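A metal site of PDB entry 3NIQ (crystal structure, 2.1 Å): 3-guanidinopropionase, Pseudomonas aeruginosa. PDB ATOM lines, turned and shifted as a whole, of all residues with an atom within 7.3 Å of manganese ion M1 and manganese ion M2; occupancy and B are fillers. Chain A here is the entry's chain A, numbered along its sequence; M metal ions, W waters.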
ATOM      1  N   ASP A 125      -2.485 -11.015  -4.290  1.00  0.00           N
ATOM      2  CA  ASP A 125      -2.907  -9.950  -5.182  1.00  0.00           C
ATOM      3  C   ASP A 125      -1.968  -8.753  -5.030  1.00  0.00           C
ATOM      4  O   ASP A 125      -1.062  -8.765  -4.193  1.00  0.00           O
ATOM      5  CB  ASP A 125      -4.381  -9.588  -4.936  1.00  0.00           C
ATOM      6  CG  ASP A 125      -4.602  -8.858  -3.591  1.00  0.00           C
ATOM      7  OD1 ASP A 125      -3.686  -8.206  -3.064  1.00  0.00           O
ATOM      8  OD2 ASP A 125      -5.722  -8.950  -3.059  1.00  0.00           O
ATOM      9  N   HIS A 126      -2.184  -7.698  -5.806  1.00  0.00           N
ATOM     10  CA  HIS A 126      -1.182  -6.630  -5.904  1.00  0.00           C
ATOM     11  C   HIS A 126      -1.094  -5.757  -4.642  1.00  0.00           C
ATOM     12  O   HIS A 126      -0.126  -5.009  -4.466  1.00  0.00           O
ATOM     13  CB  HIS A 126      -1.422  -5.747  -7.130  1.00  0.00           C
ATOM     14  CG  HIS A 126      -0.168  -5.437  -7.872  1.00  0.00           C
ATOM     15  ND1 HIS A 126      -0.118  -5.370  -9.253  1.00  0.00           N
ATOM     16  CD2 HIS A 126       1.100  -5.256  -7.439  1.00  0.00           C
ATOM     17  CE1 HIS A 126       1.127  -5.132  -9.630  1.00  0.00           C
ATOM     18  NE2 HIS A 126       1.891  -5.068  -8.549  1.00  0.00           N
ATOM     19  N   LEU A 127      -2.069  -5.884  -3.741  1.00  0.00           N
ATOM     20  CA  LEU A 127      -1.988  -5.121  -2.485  1.00  0.00           C
ATOM     21  C   LEU A 127      -0.780  -5.556  -1.668  1.00  0.00           C
ATOM     22  O   LEU A 127      -0.234  -4.780  -0.883  1.00  0.00           O
ATOM     23  CB  LEU A 127      -3.305  -5.200  -1.677  1.00  0.00           C
ATOM     24  CG  LEU A 127      -3.300  -4.402  -0.361  1.00  0.00           C
ATOM     25  CD1 LEU A 127      -3.069  -2.894  -0.636  1.00  0.00           C
ATOM     26  CD2 LEU A 127      -4.612  -4.612   0.458  1.00  0.00           C
ATOM     27  N   HIS A 146       6.659  -1.402 -13.701  1.00  0.00           N
ATOM     28  CA  HIS A 146       5.448  -2.086 -13.283  1.00  0.00           C
ATOM     29  C   HIS A 146       4.706  -2.593 -14.534  1.00  0.00           C
ATOM     30  O   HIS A 146       4.277  -1.802 -15.374  1.00  0.00           O
ATOM     31  CB  HIS A 146       4.602  -1.066 -12.503  1.00  0.00           C
ATOM     32  CG  HIS A 146       3.223  -1.532 -12.151  1.00  0.00           C
ATOM     33  ND1 HIS A 146       2.147  -0.672 -12.070  1.00  0.00           N
ATOM     34  CD2 HIS A 146       2.744  -2.770 -11.840  1.00  0.00           C
ATOM     35  CE1 HIS A 146       1.062  -1.349 -11.752  1.00  0.00           C
ATOM     36  NE2 HIS A 146       1.396  -2.626 -11.601  1.00  0.00           N
ATOM     37  N   PHE A 147       4.599  -3.899 -14.672  1.00  0.00           N
ATOM     38  CA  PHE A 147       3.911  -4.547 -15.804  1.00  0.00           C
ATOM     39  C   PHE A 147       2.491  -4.906 -15.363  1.00  0.00           C
ATOM     40  O   PHE A 147       2.338  -5.669 -14.402  1.00  0.00           O
ATOM     41  CB  PHE A 147       4.631  -5.852 -16.184  1.00  0.00           C
ATOM     42  CG  PHE A 147       6.027  -5.643 -16.669  1.00  0.00           C
ATOM     43  CD1 PHE A 147       6.293  -5.510 -18.021  1.00  0.00           C
ATOM     44  CD2 PHE A 147       7.093  -5.623 -15.770  1.00  0.00           C
ATOM     45  CE1 PHE A 147       7.605  -5.332 -18.483  1.00  0.00           C
ATOM     46  CE2 PHE A 147       8.393  -5.439 -16.217  1.00  0.00           C
ATOM     47  CZ  PHE A 147       8.654  -5.299 -17.574  1.00  0.00           C
ATOM     48  N   ASP A 148       1.477  -4.368 -16.022  1.00  0.00           N
ATOM     49  CA  ASP A 148       0.103  -4.561 -15.552  1.00  0.00           C
ATOM     50  C   ASP A 148      -0.924  -4.182 -16.616  1.00  0.00           C
ATOM     51  O   ASP A 148      -0.681  -3.277 -17.437  1.00  0.00           O
ATOM     52  CB  ASP A 148      -0.115  -3.688 -14.295  1.00  0.00           C
ATOM     53  CG  ASP A 148      -1.161  -4.252 -13.336  1.00  0.00           C
ATOM     54  OD1 ASP A 148      -2.261  -4.671 -13.762  1.00  0.00           O
ATOM     55  OD2 ASP A 148      -0.889  -4.241 -12.124  1.00  0.00           O
ATOM     56  N   ALA A 149      -2.077  -4.856 -16.607  1.00  0.00           N
ATOM     57  CA  ALA A 149      -3.219  -4.368 -17.391  1.00  0.00           C
ATOM     58  C   ALA A 149      -3.857  -3.132 -16.721  1.00  0.00           C
ATOM     59  O   ALA A 149      -4.634  -2.419 -17.373  1.00  0.00           O
ATOM     60  CB  ALA A 149      -4.261  -5.471 -17.580  1.00  0.00           C
ATOM     61  N   HIS A 150      -3.545  -2.904 -15.448  1.00  0.00           N
ATOM     62  CA  HIS A 150      -4.165  -1.827 -14.640  1.00  0.00           C
ATOM     63  C   HIS A 150      -3.137  -0.950 -13.904  1.00  0.00           C
ATOM     64  O   HIS A 150      -2.131  -1.438 -13.402  1.00  0.00           O
ATOM     65  CB  HIS A 150      -5.125  -2.429 -13.598  1.00  0.00           C
ATOM     66  CG  HIS A 150      -5.975  -3.536 -14.137  1.00  0.00           C
ATOM     67  ND1 HIS A 150      -5.626  -4.874 -14.018  1.00  0.00           N
ATOM     68  CD2 HIS A 150      -7.164  -3.513 -14.792  1.00  0.00           C
ATOM     69  CE1 HIS A 150      -6.548  -5.616 -14.598  1.00  0.00           C
ATOM     70  NE2 HIS A 150      -7.502  -4.822 -15.061  1.00  0.00           N
ATOM     71  N   SER A 151      -3.418   0.346 -13.794  1.00  0.00           N
ATOM     72  CA  SER A 151      -2.486   1.234 -13.098  1.00  0.00           C
ATOM     73  C   SER A 151      -2.425   0.984 -11.603  1.00  0.00           C
ATOM     74  O   SER A 151      -1.388   1.250 -10.973  1.00  0.00           O
ATOM     75  CB  SER A 151      -2.814   2.698 -13.405  1.00  0.00           C
ATOM     76  OG  SER A 151      -4.095   3.034 -12.915  1.00  0.00           O
ATOM     77  N   ASP A 152      -3.524   0.490 -11.003  1.00  0.00           N
ATOM     78  CA  ASP A 152      -3.564   0.214  -9.553  1.00  0.00           C
ATOM     79  C   ASP A 152      -3.268   1.477  -8.743  1.00  0.00           C
ATOM     80  O   ASP A 152      -2.570   1.441  -7.719  1.00  0.00           O
ATOM     81  CB  ASP A 152      -2.534  -0.871  -9.151  1.00  0.00           C
ATOM     82  CG  ASP A 152      -2.877  -2.241  -9.696  1.00  0.00           C
ATOM     83  OD1 ASP A 152      -3.988  -2.406 -10.221  1.00  0.00           O
ATOM     84  OD2 ASP A 152      -2.025  -3.157  -9.617  1.00  0.00           O
ATOM     85  N   HIS A 165      -6.321  -4.238  -3.959  1.00  0.00           N
ATOM     86  CA  HIS A 165      -5.311  -4.549  -4.967  1.00  0.00           C
ATOM     87  C   HIS A 165      -5.292  -3.489  -6.076  1.00  0.00           C
ATOM     88  O   HIS A 165      -4.391  -3.472  -6.903  1.00  0.00           O
ATOM     89  CB  HIS A 165      -5.514  -5.965  -5.529  1.00  0.00           C
ATOM     90  CG  HIS A 165      -6.790  -6.147  -6.300  1.00  0.00           C
ATOM     91  ND1 HIS A 165      -6.974  -7.184  -7.194  1.00  0.00           N
ATOM     92  CD2 HIS A 165      -7.935  -5.425  -6.319  1.00  0.00           C
ATOM     93  CE1 HIS A 165      -8.194  -7.105  -7.709  1.00  0.00           C
ATOM     94  NE2 HIS A 165      -8.791  -6.034  -7.199  1.00  0.00           N
ATOM     95  N   GLY A 166      -6.277  -2.591  -6.082  1.00  0.00           N
ATOM     96  CA  GLY A 166      -6.337  -1.511  -7.061  1.00  0.00           C
ATOM     97  C   GLY A 166      -5.841  -0.163  -6.547  1.00  0.00           C
ATOM     98  O   GLY A 166      -5.847   0.798  -7.295  1.00  0.00           O
ATOM     99  N   PRO A 168      -2.652   0.127  -4.481  1.00  0.00           N
ATOM    100  CA  PRO A 168      -1.379   0.122  -3.725  1.00  0.00           C
ATOM    101  C   PRO A 168      -0.377   1.216  -4.137  1.00  0.00           C
ATOM    102  O   PRO A 168       0.347   1.734  -3.290  1.00  0.00           O
ATOM    103  CB  PRO A 168      -0.820  -1.267  -3.991  1.00  0.00           C
ATOM    104  CG  PRO A 168      -1.371  -1.649  -5.347  1.00  0.00           C
ATOM    105  CD  PRO A 168      -2.774  -1.069  -5.335  1.00  0.00           C
ATOM    106  N   PHE A 169      -0.297   1.524  -5.421  1.00  0.00           N
ATOM    107  CA  PHE A 169       0.731   2.453  -5.860  1.00  0.00           C
ATOM    108  C   PHE A 169       0.348   3.899  -5.619  1.00  0.00           C
ATOM    109  O   PHE A 169       1.223   4.771  -5.535  1.00  0.00           O
ATOM    110  CB  PHE A 169       1.161   2.146  -7.308  1.00  0.00           C
ATOM    111  CG  PHE A 169       1.744   0.787  -7.433  1.00  0.00           C
ATOM    112  CD1 PHE A 169       1.177  -0.166  -8.279  1.00  0.00           C
ATOM    113  CD2 PHE A 169       2.794   0.401  -6.600  1.00  0.00           C
ATOM    114  CE1 PHE A 169       1.688  -1.467  -8.335  1.00  0.00           C
ATOM    115  CE2 PHE A 169       3.313  -0.885  -6.642  1.00  0.00           C
ATOM    116  CZ  PHE A 169       2.743  -1.835  -7.518  1.00  0.00           C
ATOM    117  N   SER A 238       7.733  -4.890 -10.463  1.00  0.00           N
ATOM    118  CA  SER A 238       6.545  -5.570 -10.041  1.00  0.00           C
ATOM    119  C   SER A 238       5.773  -6.073 -11.265  1.00  0.00           C
ATOM    120  O   SER A 238       5.343  -5.291 -12.115  1.00  0.00           O
ATOM    121  CB  SER A 238       5.694  -4.618  -9.201  1.00  0.00           C
ATOM    122  OG  SER A 238       4.516  -5.269  -8.768  1.00  0.00           O
ATOM    123  N   PHE A 239       5.558  -7.384 -11.315  1.00  0.00           N
ATOM    124  CA  PHE A 239       4.958  -8.014 -12.488  1.00  0.00           C
ATOM    125  C   PHE A 239       3.589  -8.632 -12.154  1.00  0.00           C
ATOM    126  O   PHE A 239       3.513  -9.634 -11.432  1.00  0.00           O
ATOM    127  CB  PHE A 239       5.925  -9.096 -13.017  1.00  0.00           C
ATOM    128  CG  PHE A 239       5.522  -9.657 -14.350  1.00  0.00           C
ATOM    129  CD1 PHE A 239       6.010  -9.092 -15.530  1.00  0.00           C
ATOM    130  CD2 PHE A 239       4.650 -10.743 -14.434  1.00  0.00           C
ATOM    131  CE1 PHE A 239       5.634  -9.607 -16.793  1.00  0.00           C
ATOM    132  CE2 PHE A 239       4.248 -11.256 -15.677  1.00  0.00           C
ATOM    133  CZ  PHE A 239       4.737 -10.692 -16.858  1.00  0.00           C
ATOM    134  N   ASP A 240       2.524  -8.018 -12.669  1.00  0.00           N
ATOM    135  CA  ASP A 240       1.180  -8.522 -12.474  1.00  0.00           C
ATOM    136  C   ASP A 240       0.899  -9.384 -13.723  1.00  0.00           C
ATOM    137  O   ASP A 240       0.969  -8.886 -14.841  1.00  0.00           O
ATOM    138  CB  ASP A 240       0.199  -7.338 -12.327  1.00  0.00           C
ATOM    139  CG  ASP A 240      -1.271  -7.756 -12.198  1.00  0.00           C
ATOM    140  OD1 ASP A 240      -1.647  -8.886 -12.601  1.00  0.00           O
ATOM    141  OD2 ASP A 240      -2.091  -6.935 -11.726  1.00  0.00           O
ATOM    142  N   VAL A 241       0.626 -10.668 -13.509  1.00  0.00           N
ATOM    143  CA  VAL A 241       0.516 -11.589 -14.625  1.00  0.00           C
ATOM    144  C   VAL A 241      -0.649 -11.226 -15.542  1.00  0.00           C
ATOM    145  O   VAL A 241      -0.665 -11.641 -16.683  1.00  0.00           O
ATOM    146  CB  VAL A 241       0.424 -13.081 -14.206  1.00  0.00           C
ATOM    147  CG1 VAL A 241       1.696 -13.549 -13.458  1.00  0.00           C
ATOM    148  CG2 VAL A 241      -0.835 -13.350 -13.376  1.00  0.00           C
ATOM    149  N   ASP A 242      -1.599 -10.428 -15.058  1.00  0.00           N
ATOM    150  CA  ASP A 242      -2.704 -10.010 -15.934  1.00  0.00           C
ATOM    151  C   ASP A 242      -2.262  -8.967 -17.004  1.00  0.00           C
ATOM    152  O   ASP A 242      -3.057  -8.577 -17.860  1.00  0.00           O
ATOM    153  CB  ASP A 242      -3.964  -9.598 -15.109  1.00  0.00           C
ATOM    154  CG  ASP A 242      -3.833  -8.214 -14.447  1.00  0.00           C
ATOM    155  OD1 ASP A 242      -2.998  -7.397 -14.868  1.00  0.00           O
ATOM    156  OD2 ASP A 242      -4.613  -7.950 -13.490  1.00  0.00           O
ATOM    157  N   VAL A 243      -0.992  -8.536 -16.977  1.00  0.00           N
ATOM    158  CA  VAL A 243      -0.418  -7.806 -18.122  1.00  0.00           C
ATOM    159  C   VAL A 243      -0.458  -8.701 -19.377  1.00  0.00           C
ATOM    160  O   VAL A 243      -0.645  -8.236 -20.506  1.00  0.00           O
ATOM    161  CB  VAL A 243       1.029  -7.343 -17.873  1.00  0.00           C
ATOM    162  CG1 VAL A 243       2.008  -8.520 -17.905  1.00  0.00           C
ATOM    163  CG2 VAL A 243       1.422  -6.239 -18.870  1.00  0.00           C
ATOM    164  N   THR A 252      -6.030 -15.629 -13.333  1.00  0.00           N
ATOM    165  CA  THR A 252      -5.834 -14.325 -12.710  1.00  0.00           C
ATOM    166  C   THR A 252      -7.190 -13.688 -12.441  1.00  0.00           C
ATOM    167  O   THR A 252      -8.179 -13.951 -13.153  1.00  0.00           O
ATOM    168  CB  THR A 252      -4.922 -13.412 -13.569  1.00  0.00           C
ATOM    169  OG1 THR A 252      -4.402 -12.348 -12.761  1.00  0.00           O
ATOM    170  CG2 THR A 252      -5.684 -12.852 -14.793  1.00  0.00           C
ATOM    171  N   THR A 254      -8.469 -10.521 -12.482  1.00  0.00           N
ATOM    172  CA  THR A 254      -9.055  -9.454 -13.307  1.00  0.00           C
ATOM    173  C   THR A 254      -8.516  -9.472 -14.744  1.00  0.00           C
ATOM    174  O   THR A 254      -7.786  -8.552 -15.153  1.00  0.00           O
ATOM    175  CB  THR A 254      -8.801  -8.073 -12.652  1.00  0.00           C
ATOM    176  OG1 THR A 254      -9.236  -8.128 -11.291  1.00  0.00           O
ATOM    177  CG2 THR A 254      -9.598  -6.954 -13.385  1.00  0.00           C
ATOM    178  N   GLU A 256      -8.017  -9.066 -18.734  1.00  0.00           N
ATOM    179  CA  GLU A 256      -8.414  -8.123 -19.775  1.00  0.00           C
ATOM    180  C   GLU A 256      -7.839  -8.664 -21.076  1.00  0.00           C
ATOM    181  O   GLU A 256      -6.631  -8.889 -21.158  1.00  0.00           O
ATOM    182  CB  GLU A 256      -7.806  -6.723 -19.521  1.00  0.00           C
ATOM    183  CG  GLU A 256      -8.012  -6.144 -18.110  1.00  0.00           C
ATOM    184  CD  GLU A 256      -9.426  -5.648 -17.865  1.00  0.00           C
ATOM    185  OE1 GLU A 256     -10.202  -5.536 -18.845  1.00  0.00           O
ATOM    186  OE2 GLU A 256      -9.765  -5.353 -16.685  1.00  0.00           O
ATOM    187  N   VAL A 283       2.822 -11.054  -9.109  1.00  0.00           N
ATOM    188  CA  VAL A 283       1.577 -11.072  -8.331  1.00  0.00           C
ATOM    189  C   VAL A 283       0.392 -11.452  -9.199  1.00  0.00           C
ATOM    190  O   VAL A 283       0.516 -11.482 -10.406  1.00  0.00           O
ATOM    191  CB  VAL A 283       1.312  -9.700  -7.677  1.00  0.00           C
ATOM    192  CG1 VAL A 283       2.414  -9.377  -6.697  1.00  0.00           C
ATOM    193  CG2 VAL A 283       1.144  -8.582  -8.757  1.00  0.00           C
ATOM    194  N   GLU A 284      -0.721 -11.767  -8.529  1.00  0.00           N
ATOM    195  CA  GLU A 284      -2.051 -12.035  -9.126  1.00  0.00           C
ATOM    196  C   GLU A 284      -2.160 -13.414  -9.812  1.00  0.00           C
ATOM    197  O   GLU A 284      -3.138 -13.652 -10.537  1.00  0.00           O
ATOM    198  CB  GLU A 284      -2.519 -10.893 -10.082  1.00  0.00           C
ATOM    199  CG  GLU A 284      -2.694  -9.508  -9.426  1.00  0.00           C
ATOM    200  CD  GLU A 284      -3.901  -9.434  -8.478  1.00  0.00           C
ATOM    201  OE1 GLU A 284      -4.656 -10.426  -8.343  1.00  0.00           O
ATOM    202  OE2 GLU A 284      -4.071  -8.383  -7.832  1.00  0.00           O
HETATM  203 MN    MN M   1      -3.725  -5.931 -12.981  1.00  0.00          MN
HETATM  204 MN    MN M   2      -1.980  -5.183 -10.453  1.00  0.00          MN
HETATM  205  O   HOH W   1      -4.269  -4.801 -11.133  1.00  0.00           O
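The side-chain carboxylate (OD1) of Asp 242 lies close to the backbone NH (N) of Ala 149, 3.2 Å away.
O of Asp 152 sits at hydrogen-bond distance from N of Phe 169, 3.2 Å away.
The backbone NH (N) of His 126 lies within hydrogen-bond range of the side-chain carboxylate (OE2) of Glu 284, 2.9 Å away.
The side-chain carboxylate of Glu 256 lies within hydrogen-bond range of a ring nitrogen (NE2) of His 150 (2.8 Å).
NE2 of His 126 is in hydrogen-bond range of OG of Ser 238 (2.6 Å).
The side-chain carboxylate of Asp 148 lies close to a ring nitrogen (NE2) of His 146.
The backbone carbonyl oxygen of Phe 147 is in hydrogen-bond range of the backbone NH of Asp 240.
Within 4 Å of manganese ion M1: Asp 148, His 150, Asp 240 and Asp 242.
The nearest printed residue that does not touch manganese ion M1 is Ala 149 (4.1 Å).
Of the 25 residues printed, 4 come within 4 Å of manganese ion M2.
The nearest printed residue that does not touch manganese ion M2 is His 146 (4.4 Å).
Manganese ion M1 is bound by the side-chain carboxylate (OD1) of Asp 148 (2.1 Å), water W1 (2.2 Å), the side-chain carboxylate (OD2) of Asp 242 (2.3 Å), the side-chain carboxylate (OD2) of Asp 240 (2.3 Å), a ring nitrogen (ND1) of His 150 (2.4 Å) and the side-chain carboxylate (OD1) of Asp 242 (2.5 Å).
Manganese ion M2 is bound by the side-chain carboxylate (OD2) of Asp 240 (2.2 Å).
OD2 of Asp 152 binds manganese ion M2, 2.2 Å away.
Manganese ion M2 is bound by OD2 of Asp 148 (2.2 Å).
ND1 of His 126 binds manganese ion M2, at 2.2 Å.
Manganese ion M2 is bound by water W1 (2.4 Å).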
